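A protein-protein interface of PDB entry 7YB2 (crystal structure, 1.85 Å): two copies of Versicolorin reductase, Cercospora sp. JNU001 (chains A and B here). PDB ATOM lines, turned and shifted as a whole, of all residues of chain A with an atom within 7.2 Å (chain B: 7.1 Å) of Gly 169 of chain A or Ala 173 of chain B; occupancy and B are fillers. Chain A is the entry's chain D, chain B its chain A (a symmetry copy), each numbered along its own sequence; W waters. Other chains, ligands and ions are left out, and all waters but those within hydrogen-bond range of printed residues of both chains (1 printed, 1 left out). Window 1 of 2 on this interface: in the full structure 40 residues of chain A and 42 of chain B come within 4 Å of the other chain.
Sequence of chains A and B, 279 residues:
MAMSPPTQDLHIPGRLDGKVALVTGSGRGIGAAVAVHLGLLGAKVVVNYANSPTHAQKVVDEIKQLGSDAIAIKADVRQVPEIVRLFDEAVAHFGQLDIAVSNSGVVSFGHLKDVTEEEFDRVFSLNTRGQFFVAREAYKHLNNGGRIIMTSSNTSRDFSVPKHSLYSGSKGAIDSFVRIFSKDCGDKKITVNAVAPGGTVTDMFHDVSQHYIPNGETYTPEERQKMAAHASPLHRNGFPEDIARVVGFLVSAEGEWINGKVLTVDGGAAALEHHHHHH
The side-chain carboxylate of Asp 175 of chain B is in salt-bridge range of the guanidinium group of Arg 157 of chain A (2.8 Å). The side-chain hydroxyl (OG) of Ser 176 of chain A is in hydrogen-bond range of the backbone carbonyl oxygen (O) of Ser 156 of chain B (2.7 Å). The backbone carbonyl oxygen (O) of Ser 156 of chain A is in hydrogen-bond range of the side-chain hydroxyl (OG) of Ser 176 of chain B (2.7 Å).
Printed residues of chain B that touch a printed residue of chain A: Phe 124, Thr 128, Ser 156, Ser 168, Gly 169, Gly 172, Ala 173, Asp 175, Ser 176, Phe 177 and Ile 180. Hydrophobic or aromatic side chains of chain B within 4 Å of the printed part of chain A: Phe 124, Ala 173, Phe 177 and Ile 180. Among the printed residues, Asp or Glu carboxylates within 4 Å of a Lys or Arg side-chain nitrogen of the other chain: Arg 157 of chain A with Asp 175 of chain B (2.8 Å).
Water W1 lies within hydrogen-bond range of O of Ser 156 of chain A (3.1 Å), NH1 of Arg 157 of chain A (3.3 Å), OG of Ser 176 of chain B (3.4 Å) and O of Asp 175 of chain B (3.5 Å).
OG of Ser 156 of chain B is in hydrogen-bond range of OD2 of Asp 175 of chain B, at 2.7 Å. OG of Ser 168 of chain A sits at hydrogen-bond distance from O of His 164 of chain A. OG of Ser 168 of chain A is in hydrogen-bond range of O of Thr 155 of chain A. The backbone carbonyl oxygen of Ser 170 of chain A sits at hydrogen-bond distance from the side-chain hydroxyl of Thr 128 of chain A (2.8 Å). The side-chain hydroxyl of Thr 128 of chain B sits at hydrogen-bond distance from the backbone carbonyl oxygen of Ser 170 of chain B, at 2.7 Å. The side-chain hydroxyl (OG) of Ser 152 of chain B sits at hydrogen-bond distance from the side-chain carboxylate (OD1) of Asp 175 of chain B (2.5 Å).
Gly 169 of chain A touches Ala 173 of chain B, and with the chains exchanged Ala 173 of chain A touches Gly 169 of chain B. Gly 169 of chain A touches Ser 176 of chain B, and with the chains exchanged Ser 176 of chain A touches Gly 169 of chain B. Gly 172 of chain A touches its own counterpart, Gly 172 of chain B. Ala 173 of chain A touches its own counterpart, Ala 173 of chain B. Positions printed for both chains: 124, 128, 156, 168, 169, 170, 171, 172, 173, 174 and 176.
Among the printed residues, pairs that only touch across the chains: Phe 124 of chain A with Thr 128 of chain B, Phe 124 of chain A with Phe 177 of chain B, Thr 128 of chain A with Phe 124 of chain B, His 164 of chain A with Ile 180 of chain B, Ser 165 of chain A with Phe 177 of chain B, Ser 165 of chain A with Ile 180 of chain B, Ser 168 of chain A with Ser 176 of chain B, Ser 168 of chain A with Ile 180 of chain B, Gly 169 of chain A with Ala 173 of chain B, Gly 169 of chain A with Ser 176 of chain B, Gly 169 of chain A with Phe 177 of chain B, Gly 172 of chain A with Gly 172 of chain B, Gly 172 of chain A with Ser 176 of chain B, Ala 173 of chain A with Gly 169 of chain B, Ala 173 of chain A with Ala 173 of chain B, Ser 176 of chain A with Ser 168 of chain B, Ser 176 of chain A with Gly 169 of chain B and Ser 176 of chain A with Gly 172 of chain B.
Of the printed residues of chain B, Arg 157 of chain A touches Asp 175. Of the printed residues of chain B, His 164 of chain A touches Ile 180. Of chain B, only Ala 173, Ser 176 and Phe 177 come within 4 Å of Gly 169 of chain A. Ser 170 of chain A touches none of the printed residues of chain B. Lys 171 of chain A touches none of the printed residues of chain B. Printed residues of chain B within 4 Å of Gly 172 of chain A: Gly 172 and Ser 176. Of the printed residues of chain A, Thr 128 of chain B touches Phe 124 (3.7 Å). Of the printed residues of chain A, Ser 168 of chain B touches Ser 176 (3.5 Å). Of chain A, only Gly 172 (3.9 Å) and Ser 176 (3.3 Å) come within 4 Å of Gly 172 of chain B. The nearest residue of chain B that does not touch Gly 169 of chain A is Gly 172 of chain B (5.1 Å). The nearest residue of chain A that does not touch Ala 173 of chain B is Gly 172 of chain A (4.1 Å).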
ATOM      1  N   PHE A 120      19.758  23.699 -39.713  1.00  0.00           N
ATOM      2  CA  PHE A 120      20.040  23.146 -38.368  1.00  0.00           C
ATOM      3  C   PHE A 120      21.314  22.292 -38.453  1.00  0.00           C
ATOM      4  O   PHE A 120      22.259  22.511 -37.702  1.00  0.00           O
ATOM      5  CB  PHE A 120      18.853  22.366 -37.829  1.00  0.00           C
ATOM      6  CG  PHE A 120      19.120  21.862 -36.427  1.00  0.00           C
ATOM      7  CD1 PHE A 120      20.037  20.858 -36.196  1.00  0.00           C
ATOM      8  CD2 PHE A 120      18.503  22.472 -35.332  1.00  0.00           C
ATOM      9  CE1 PHE A 120      20.331  20.452 -34.899  1.00  0.00           C
ATOM     10  CE2 PHE A 120      18.774  22.045 -34.046  1.00  0.00           C
ATOM     11  CZ  PHE A 120      19.702  21.058 -33.829  1.00  0.00           C
ATOM     12  N   VAL A 123      24.722  24.132 -39.153  1.00  0.00           N
ATOM     13  CA  VAL A 123      25.227  24.878 -37.966  1.00  0.00           C
ATOM     14  C   VAL A 123      25.731  23.912 -36.871  1.00  0.00           C
ATOM     15  O   VAL A 123      26.889  24.034 -36.406  1.00  0.00           O
ATOM     16  CB  VAL A 123      24.170  25.873 -37.451  1.00  0.00           C
ATOM     17  CG1 VAL A 123      24.628  26.513 -36.150  1.00  0.00           C
ATOM     18  CG2 VAL A 123      23.885  26.962 -38.477  1.00  0.00           C
ATOM     19  N   PHE A 124      24.933  22.933 -36.485  1.00  0.00           N
ATOM     20  CA  PHE A 124      25.297  22.020 -35.375  1.00  0.00           C
ATOM     21  C   PHE A 124      26.459  21.124 -35.785  1.00  0.00           C
ATOM     22  O   PHE A 124      27.291  20.783 -34.942  1.00  0.00           O
ATOM     23  CB  PHE A 124      24.071  21.264 -34.866  1.00  0.00           C
ATOM     24  CG  PHE A 124      23.418  21.980 -33.708  1.00  0.00           C
ATOM     25  CD1 PHE A 124      22.723  23.161 -33.909  1.00  0.00           C
ATOM     26  CD2 PHE A 124      23.464  21.448 -32.424  1.00  0.00           C
ATOM     27  CE1 PHE A 124      22.072  23.793 -32.860  1.00  0.00           C
ATOM     28  CE2 PHE A 124      22.851  22.102 -31.361  1.00  0.00           C
ATOM     29  CZ  PHE A 124      22.187  23.287 -31.575  1.00  0.00           C
ATOM     30  N   THR A 128      28.898  22.455 -32.883  1.00  0.00           N
ATOM     31  CA  THR A 128      28.544  21.696 -31.670  1.00  0.00           C
ATOM     32  C   THR A 128      29.150  20.310 -31.768  1.00  0.00           C
ATOM     33  O   THR A 128      30.016  19.975 -30.966  1.00  0.00           O
ATOM     34  CB  THR A 128      27.027  21.696 -31.444  1.00  0.00           C
ATOM     35  OG1 THR A 128      26.552  23.035 -31.526  1.00  0.00           O
ATOM     36  CG2 THR A 128      26.708  21.049 -30.109  1.00  0.00           C
ATOM     37  N   THR A 155      26.212  35.282 -27.161  1.00  0.00           N
ATOM     38  CA  THR A 155      24.809  34.958 -27.543  1.00  0.00           C
ATOM     39  C   THR A 155      24.283  33.690 -26.851  1.00  0.00           C
ATOM     40  O   THR A 155      23.055  33.533 -26.853  1.00  0.00           O
ATOM     41  CB  THR A 155      24.648  34.849 -29.055  1.00  0.00           C
ATOM     42  OG1 THR A 155      25.437  33.754 -29.503  1.00  0.00           O
ATOM     43  CG2 THR A 155      25.009  36.144 -29.760  1.00  0.00           C
ATOM     44  N   SER A 156      25.136  32.837 -26.267  1.00  0.00           N
ATOM     45  CA  SER A 156      24.675  31.591 -25.619  1.00  0.00           C
ATOM     46  C   SER A 156      23.814  31.926 -24.393  1.00  0.00           C
ATOM     47  O   SER A 156      22.791  31.294 -24.228  1.00  0.00           O
ATOM     48  CB  SER A 156      25.801  30.661 -25.268  1.00  0.00           C
ATOM     49  OG  SER A 156      26.602  31.178 -24.241  1.00  0.00           O
ATOM     50  N   ARG A 157      24.208  32.915 -23.608  1.00  0.00           N
ATOM     51  CA  ARG A 157      23.614  33.203 -22.266  1.00  0.00           C
ATOM     52  C   ARG A 157      23.387  34.712 -22.071  1.00  0.00           C
ATOM     53  O   ARG A 157      22.382  35.044 -21.522  1.00  0.00           O
ATOM     54  CB  ARG A 157      24.539  32.702 -21.146  1.00  0.00           C
ATOM     55  CG  ARG A 157      24.630  31.184 -20.990  1.00  0.00           C
ATOM     56  CD  ARG A 157      23.460  30.533 -20.234  1.00  0.00           C
ATOM     57  NE  ARG A 157      23.473  29.052 -20.243  1.00  0.00           N
ATOM     58  CZ  ARG A 157      22.512  28.252 -19.741  1.00  0.00           C
ATOM     59  NH1 ARG A 157      21.434  28.786 -19.175  1.00  0.00           N
ATOM     60  NH2 ARG A 157      22.632  26.919 -19.844  1.00  0.00           N
ATOM     61  N   HIS A 164      18.065  34.450 -33.797  1.00  0.00           N
ATOM     62  CA  HIS A 164      19.415  33.898 -33.584  1.00  0.00           C
ATOM     63  C   HIS A 164      19.371  32.595 -32.766  1.00  0.00           C
ATOM     64  O   HIS A 164      20.390  32.259 -32.186  1.00  0.00           O
ATOM     65  CB  HIS A 164      20.223  35.000 -32.943  1.00  0.00           C
ATOM     66  CG  HIS A 164      21.683  34.919 -33.200  1.00  0.00           C
ATOM     67  ND1 HIS A 164      22.218  34.419 -34.390  1.00  0.00           N
ATOM     68  CD2 HIS A 164      22.715  35.392 -32.481  1.00  0.00           C
ATOM     69  CE1 HIS A 164      23.520  34.591 -34.347  1.00  0.00           C
ATOM     70  NE2 HIS A 164      23.857  35.179 -33.206  1.00  0.00           N
ATOM     71  N   SER A 165      18.252  31.886 -32.761  1.00  0.00           N
ATOM     72  CA  SER A 165      18.025  30.726 -31.868  1.00  0.00           C
ATOM     73  C   SER A 165      18.960  29.583 -32.229  1.00  0.00           C
ATOM     74  O   SER A 165      19.614  29.026 -31.315  1.00  0.00           O
ATOM     75  CB  SER A 165      16.572  30.285 -31.888  1.00  0.00           C
ATOM     76  OG  SER A 165      16.179  29.768 -33.157  1.00  0.00           O
ATOM     77  N   LEU A 166      19.041  29.253 -33.519  1.00  0.00           N
ATOM     78  CA  LEU A 166      19.852  28.098 -33.951  1.00  0.00           C
ATOM     79  C   LEU A 166      21.315  28.282 -33.509  1.00  0.00           C
ATOM     80  O   LEU A 166      21.905  27.347 -32.926  1.00  0.00           O
ATOM     81  CB  LEU A 166      19.798  27.970 -35.471  1.00  0.00           C
ATOM     82  CG  LEU A 166      20.542  26.772 -36.031  1.00  0.00           C
ATOM     83  CD1 LEU A 166      20.023  25.463 -35.444  1.00  0.00           C
ATOM     84  CD2 LEU A 166      20.417  26.772 -37.556  1.00  0.00           C
ATOM     85  N   TYR A 167      21.925  29.415 -33.869  1.00  0.00           N
ATOM     86  CA  TYR A 167      23.339  29.703 -33.522  1.00  0.00           C
ATOM     87  C   TYR A 167      23.501  29.757 -31.991  1.00  0.00           C
ATOM     88  O   TYR A 167      24.423  29.118 -31.430  1.00  0.00           O
ATOM     89  CB  TYR A 167      23.765  31.008 -34.177  1.00  0.00           C
ATOM     90  CG  TYR A 167      25.165  31.407 -33.868  1.00  0.00           C
ATOM     91  CD1 TYR A 167      26.224  30.878 -34.586  1.00  0.00           C
ATOM     92  CD2 TYR A 167      25.426  32.309 -32.871  1.00  0.00           C
ATOM     93  CE1 TYR A 167      27.523  31.249 -34.308  1.00  0.00           C
ATOM     94  CE2 TYR A 167      26.714  32.688 -32.569  1.00  0.00           C
ATOM     95  CZ  TYR A 167      27.765  32.170 -33.306  1.00  0.00           C
ATOM     96  OH  TYR A 167      29.031  32.595 -33.030  1.00  0.00           O
ATOM     97  N   SER A 168      22.616  30.467 -31.289  1.00  0.00           N
ATOM     98  CA  SER A 168      22.730  30.660 -29.817  1.00  0.00           C
ATOM     99  C   SER A 168      22.739  29.282 -29.140  1.00  0.00           C
ATOM    100  O   SER A 168      23.611  29.061 -28.276  1.00  0.00           O
ATOM    101  CB  SER A 168      21.656  31.539 -29.286  1.00  0.00           C
ATOM    102  OG  SER A 168      21.797  32.827 -29.865  1.00  0.00           O
ATOM    103  N   GLY A 169      21.867  28.376 -29.581  1.00  0.00           N
ATOM    104  CA  GLY A 169      21.757  26.999 -29.065  1.00  0.00           C
ATOM    105  C   GLY A 169      23.001  26.179 -29.355  1.00  0.00           C
ATOM    106  O   GLY A 169      23.479  25.460 -28.448  1.00  0.00           O
ATOM    107  N   SER A 170      23.579  26.326 -30.562  1.00  0.00           N
ATOM    108  CA  SER A 170      24.819  25.621 -30.957  1.00  0.00           C
ATOM    109  C   SER A 170      25.941  25.971 -29.970  1.00  0.00           C
ATOM    110  O   SER A 170      26.748  25.076 -29.670  1.00  0.00           O
ATOM    111  CB  SER A 170      25.190  25.919 -32.433  1.00  0.00           C
ATOM    112  OG  SER A 170      25.850  27.195 -32.536  1.00  0.00           O
ATOM    113  N   LYS A 171      25.979  27.192 -29.432  1.00  0.00           N
ATOM    114  CA  LYS A 171      27.006  27.686 -28.475  1.00  0.00           C
ATOM    115  C   LYS A 171      26.638  27.366 -27.027  1.00  0.00           C
ATOM    116  O   LYS A 171      27.545  27.080 -26.236  1.00  0.00           O
ATOM    117  CB  LYS A 171      27.254  29.178 -28.715  1.00  0.00           C
ATOM    118  CG  LYS A 171      27.728  29.507 -30.145  1.00  0.00           C
ATOM    119  CD  LYS A 171      28.952  28.740 -30.576  1.00  0.00           C
ATOM    120  CE  LYS A 171      29.576  29.464 -31.756  1.00  0.00           C
ATOM    121  NZ  LYS A 171      31.014  29.255 -31.782  1.00  0.00           N
ATOM    122  N   GLY A 172      25.355  27.391 -26.674  1.00  0.00           N
ATOM    123  CA  GLY A 172      24.893  26.992 -25.335  1.00  0.00           C
ATOM    124  C   GLY A 172      25.341  25.563 -25.027  1.00  0.00           C
ATOM    125  O   GLY A 172      25.676  25.292 -23.854  1.00  0.00           O
ATOM    126  N   ALA A 173      25.325  24.653 -26.006  1.00  0.00           N
ATOM    127  CA  ALA A 173      25.795  23.262 -25.809  1.00  0.00           C
ATOM    128  C   ALA A 173      27.253  23.306 -25.351  1.00  0.00           C
ATOM    129  O   ALA A 173      27.647  22.501 -24.456  1.00  0.00           O
ATOM    130  CB  ALA A 173      25.648  22.427 -27.046  1.00  0.00           C
ATOM    131  N   ILE A 174      28.043  24.205 -25.943  1.00  0.00           N
ATOM    132  CA  ILE A 174      29.506  24.279 -25.681  1.00  0.00           C
ATOM    133  C   ILE A 174      29.744  24.646 -24.217  1.00  0.00           C
ATOM    134  O   ILE A 174      30.684  24.056 -23.543  1.00  0.00           O
ATOM    135  CB  ILE A 174      30.179  25.288 -26.627  1.00  0.00           C
ATOM    136  CG1 ILE A 174      30.022  24.864 -28.091  1.00  0.00           C
ATOM    137  CG2 ILE A 174      31.640  25.474 -26.235  1.00  0.00           C
ATOM    138  CD1 ILE A 174      30.517  23.478 -28.397  1.00  0.00           C
ATOM    139  N   SER A 176      27.978  23.988 -21.649  1.00  0.00           N
ATOM    140  CA  SER A 176      27.698  22.772 -20.845  1.00  0.00           C
ATOM    141  C   SER A 176      28.820  21.743 -21.044  1.00  0.00           C
ATOM    142  O   SER A 176      29.298  21.128 -20.053  1.00  0.00           O
ATOM    143  CB  SER A 176      26.329  22.215 -21.168  1.00  0.00           C
ATOM    144  OG  SER A 176      25.333  23.163 -20.866  1.00  0.00           O
ATOM    145  N   PHE B 124      21.567  13.855 -29.483  1.00  0.00           N
ATOM    146  CA  PHE B 124      21.250  15.194 -30.048  1.00  0.00           C
ATOM    147  C   PHE B 124      20.057  15.116 -30.992  1.00  0.00           C
ATOM    148  O   PHE B 124      19.254  16.054 -31.004  1.00  0.00           O
ATOM    149  CB  PHE B 124      22.488  15.796 -30.717  1.00  0.00           C
ATOM    150  CG  PHE B 124      23.275  16.670 -29.780  1.00  0.00           C
ATOM    151  CD1 PHE B 124      23.960  16.130 -28.702  1.00  0.00           C
ATOM    152  CD2 PHE B 124      23.223  18.054 -29.914  1.00  0.00           C
ATOM    153  CE1 PHE B 124      24.681  16.951 -27.852  1.00  0.00           C
ATOM    154  CE2 PHE B 124      23.915  18.873 -29.029  1.00  0.00           C
ATOM    155  CZ  PHE B 124      24.635  18.313 -28.004  1.00  0.00           C
ATOM    156  N   ASN B 127      17.034  14.968 -28.230  1.00  0.00           N
ATOM    157  CA  ASN B 127      17.004  15.926 -27.097  1.00  0.00           C
ATOM    158  C   ASN B 127      17.135  17.380 -27.566  1.00  0.00           C
ATOM    159  O   ASN B 127      16.732  18.273 -26.804  1.00  0.00           O
ATOM    160  CB  ASN B 127      18.197  15.667 -26.159  1.00  0.00           C
ATOM    161  CG  ASN B 127      18.087  14.383 -25.346  1.00  0.00           C
ATOM    162  OD1 ASN B 127      17.132  13.614 -25.493  1.00  0.00           O
ATOM    163  ND2 ASN B 127      19.018  14.196 -24.409  1.00  0.00           N
ATOM    164  N   THR B 128      17.809  17.612 -28.699  1.00  0.00           N
ATOM    165  CA  THR B 128      18.200  18.970 -29.136  1.00  0.00           C
ATOM    166  C   THR B 128      17.512  19.277 -30.482  1.00  0.00           C
ATOM    167  O   THR B 128      16.699  20.210 -30.570  1.00  0.00           O
ATOM    168  CB  THR B 128      19.717  19.120 -29.179  1.00  0.00           C
ATOM    169  OG1 THR B 128      20.238  18.666 -27.926  1.00  0.00           O
ATOM    170  CG2 THR B 128      20.079  20.558 -29.483  1.00  0.00           C
ATOM    171  N   MET B 150       9.785  23.595 -23.229  1.00  0.00           N
ATOM    172  CA  MET B 150      10.843  22.651 -23.625  1.00  0.00           C
ATOM    173  C   MET B 150      11.450  22.070 -22.350  1.00  0.00           C
ATOM    174  O   MET B 150      11.157  22.588 -21.254  1.00  0.00           O
ATOM    175  CB  MET B 150      11.860  23.379 -24.503  1.00  0.00           C
ATOM    176  CG  MET B 150      11.183  24.006 -25.732  1.00  0.00           C
ATOM    177  SD  MET B 150      12.449  24.781 -26.746  1.00  0.00           S
ATOM    178  CE  MET B 150      13.011  23.291 -27.560  1.00  0.00           C
ATOM    179  N   SER B 152      14.737  20.838 -20.253  1.00  0.00           N
ATOM    180  CA  SER B 152      16.184  20.882 -20.037  1.00  0.00           C
ATOM    181  C   SER B 152      16.519  19.912 -18.904  1.00  0.00           C
ATOM    182  O   SER B 152      15.888  18.836 -18.778  1.00  0.00           O
ATOM    183  CB  SER B 152      16.566  22.321 -19.740  1.00  0.00           C
ATOM    184  OG  SER B 152      17.970  22.435 -19.612  1.00  0.00           O
ATOM    185  N   SER B 156      22.441  20.863 -17.111  1.00  0.00           N
ATOM    186  CA  SER B 156      22.895  21.762 -18.208  1.00  0.00           C
ATOM    187  C   SER B 156      23.792  22.854 -17.616  1.00  0.00           C
ATOM    188  O   SER B 156      24.748  23.242 -18.270  1.00  0.00           O
ATOM    189  CB  SER B 156      21.725  22.346 -18.947  1.00  0.00           C
ATOM    190  OG  SER B 156      21.047  23.214 -18.088  1.00  0.00           O
ATOM    191  N   SER B 168      24.456  16.628 -20.996  1.00  0.00           N
ATOM    192  CA  SER B 168      24.431  17.989 -20.394  1.00  0.00           C
ATOM    193  C   SER B 168      24.417  19.012 -21.531  1.00  0.00           C
ATOM    194  O   SER B 168      23.679  20.019 -21.468  1.00  0.00           O
ATOM    195  CB  SER B 168      25.596  18.224 -19.452  1.00  0.00           C
ATOM    196  OG  SER B 168      25.491  17.325 -18.319  1.00  0.00           O
ATOM    197  N   GLY B 169      25.211  18.765 -22.575  1.00  0.00           N
ATOM    198  CA  GLY B 169      25.277  19.704 -23.716  1.00  0.00           C
ATOM    199  C   GLY B 169      23.999  19.710 -24.515  1.00  0.00           C
ATOM    200  O   GLY B 169      23.566  20.791 -24.960  1.00  0.00           O
ATOM    201  N   SER B 170      23.375  18.539 -24.660  1.00  0.00           N
ATOM    202  CA  SER B 170      22.094  18.393 -25.391  1.00  0.00           C
ATOM    203  C   SER B 170      21.075  19.342 -24.764  1.00  0.00           C
ATOM    204  O   SER B 170      20.290  19.958 -25.522  1.00  0.00           O
ATOM    205  CB  SER B 170      21.622  16.943 -25.452  1.00  0.00           C
ATOM    206  OG  SER B 170      21.009  16.505 -24.251  1.00  0.00           O
ATOM    207  N   LYS B 171      21.098  19.467 -23.419  1.00  0.00           N
ATOM    208  CA  LYS B 171      20.141  20.298 -22.658  1.00  0.00           C
ATOM    209  C   LYS B 171      20.624  21.737 -22.571  1.00  0.00           C
ATOM    210  O   LYS B 171      19.749  22.599 -22.550  1.00  0.00           O
ATOM    211  CB  LYS B 171      19.893  19.692 -21.280  1.00  0.00           C
ATOM    212  CG  LYS B 171      19.325  18.291 -21.352  1.00  0.00           C
ATOM    213  CD  LYS B 171      18.145  18.224 -22.280  1.00  0.00           C
ATOM    214  CE  LYS B 171      17.461  16.885 -22.315  1.00  0.00           C
ATOM    215  NZ  LYS B 171      16.249  16.876 -21.501  1.00  0.00           N
ATOM    216  N   GLY B 172      21.946  21.996 -22.526  1.00  0.00           N
ATOM    217  CA  GLY B 172      22.457  23.377 -22.554  1.00  0.00           C
ATOM    218  C   GLY B 172      21.977  24.125 -23.793  1.00  0.00           C
ATOM    219  O   GLY B 172      21.666  25.339 -23.687  1.00  0.00           O
ATOM    220  N   ALA B 173      21.878  23.455 -24.943  1.00  0.00           N
ATOM    221  CA  ALA B 173      21.346  24.048 -26.192  1.00  0.00           C
ATOM    222  C   ALA B 173      19.911  24.515 -25.957  1.00  0.00           C
ATOM    223  O   ALA B 173      19.543  25.607 -26.485  1.00  0.00           O
ATOM    224  CB  ALA B 173      21.437  23.032 -27.317  1.00  0.00           C
ATOM    225  N   ILE B 174      19.108  23.708 -25.220  1.00  0.00           N
ATOM    226  CA  ILE B 174      17.671  24.007 -24.948  1.00  0.00           C
ATOM    227  C   ILE B 174      17.559  25.339 -24.186  1.00  0.00           C
ATOM    228  O   ILE B 174      16.703  26.180 -24.529  1.00  0.00           O
ATOM    229  CB  ILE B 174      16.958  22.862 -24.210  1.00  0.00           C
ATOM    230  CG1 ILE B 174      17.046  21.564 -25.011  1.00  0.00           C
ATOM    231  CG2 ILE B 174      15.517  23.239 -23.876  1.00  0.00           C
ATOM    232  CD1 ILE B 174      16.565  21.672 -26.468  1.00  0.00           C
ATOM    233  N   ASP B 175      18.380  25.543 -23.170  1.00  0.00           N
ATOM    234  CA  ASP B 175      18.347  26.757 -22.332  1.00  0.00           C
ATOM    235  C   ASP B 175      18.534  27.978 -23.238  1.00  0.00           C
ATOM    236  O   ASP B 175      17.780  28.986 -23.065  1.00  0.00           O
ATOM    237  CB  ASP B 175      19.407  26.729 -21.233  1.00  0.00           C
ATOM    238  CG  ASP B 175      19.295  25.590 -20.238  1.00  0.00           C
ATOM    239  OD1 ASP B 175      18.330  24.841 -20.316  1.00  0.00           O
ATOM    240  OD2 ASP B 175      20.240  25.443 -19.415  1.00  0.00           O
ATOM    241  N   SER B 176      19.445  27.908 -24.220  1.00  0.00           N
ATOM    242  CA  SER B 176      19.680  29.038 -25.161  1.00  0.00           C
ATOM    243  C   SER B 176      18.496  29.167 -26.123  1.00  0.00           C
ATOM    244  O   SER B 176      18.008  30.299 -26.350  1.00  0.00           O
ATOM    245  CB  SER B 176      21.027  28.880 -25.899  1.00  0.00           C
ATOM    246  OG  SER B 176      22.105  28.832 -24.967  1.00  0.00           O
ATOM    247  N   PHE B 177      17.994  28.048 -26.651  1.00  0.00           N
ATOM    248  CA  PHE B 177      16.838  28.095 -27.569  1.00  0.00           C
ATOM    249  C   PHE B 177      15.700  28.879 -26.904  1.00  0.00           C
ATOM    250  O   PHE B 177      15.188  29.792 -27.556  1.00  0.00           O
ATOM    251  CB  PHE B 177      16.292  26.725 -27.969  1.00  0.00           C
ATOM    252  CG  PHE B 177      17.183  25.899 -28.859  1.00  0.00           C
ATOM    253  CD1 PHE B 177      18.118  26.474 -29.710  1.00  0.00           C
ATOM    254  CD2 PHE B 177      17.041  24.523 -28.864  1.00  0.00           C
ATOM    255  CE1 PHE B 177      18.894  25.676 -30.541  1.00  0.00           C
ATOM    256  CE2 PHE B 177      17.859  23.724 -29.663  1.00  0.00           C
ATOM    257  CZ  PHE B 177      18.759  24.307 -30.513  1.00  0.00           C
ATOM    258  N   VAL B 178      15.310  28.550 -25.665  1.00  0.00           N
ATOM    259  CA  VAL B 178      14.064  29.139 -25.118  1.00  0.00           C
ATOM    260  C   VAL B 178      14.195  30.660 -25.029  1.00  0.00           C
ATOM    261  O   VAL B 178      13.176  31.377 -25.190  1.00  0.00           O
ATOM    262  CB  VAL B 178      13.597  28.522 -23.790  1.00  0.00           C
ATOM    263  CG1 VAL B 178      13.355  27.024 -23.928  1.00  0.00           C
ATOM    264  CG2 VAL B 178      14.463  28.872 -22.611  1.00  0.00           C
ATOM    265  N   ILE B 180      15.840  32.847 -26.922  1.00  0.00           N
ATOM    266  CA  ILE B 180      15.677  33.500 -28.254  1.00  0.00           C
ATOM    267  C   ILE B 180      14.295  33.161 -28.826  1.00  0.00           C
ATOM    268  O   ILE B 180      13.645  34.068 -29.425  1.00  0.00           O
ATOM    269  CB  ILE B 180      16.806  33.079 -29.206  1.00  0.00           C
ATOM    270  CG1 ILE B 180      18.210  33.252 -28.608  1.00  0.00           C
ATOM    271  CG2 ILE B 180      16.609  33.768 -30.547  1.00  0.00           C
ATOM    272  CD1 ILE B 180      18.428  34.450 -27.769  1.00  0.00           C
HETATM  273  O   HOH W   1      20.876  30.203 -22.070  1.00  0.00           O
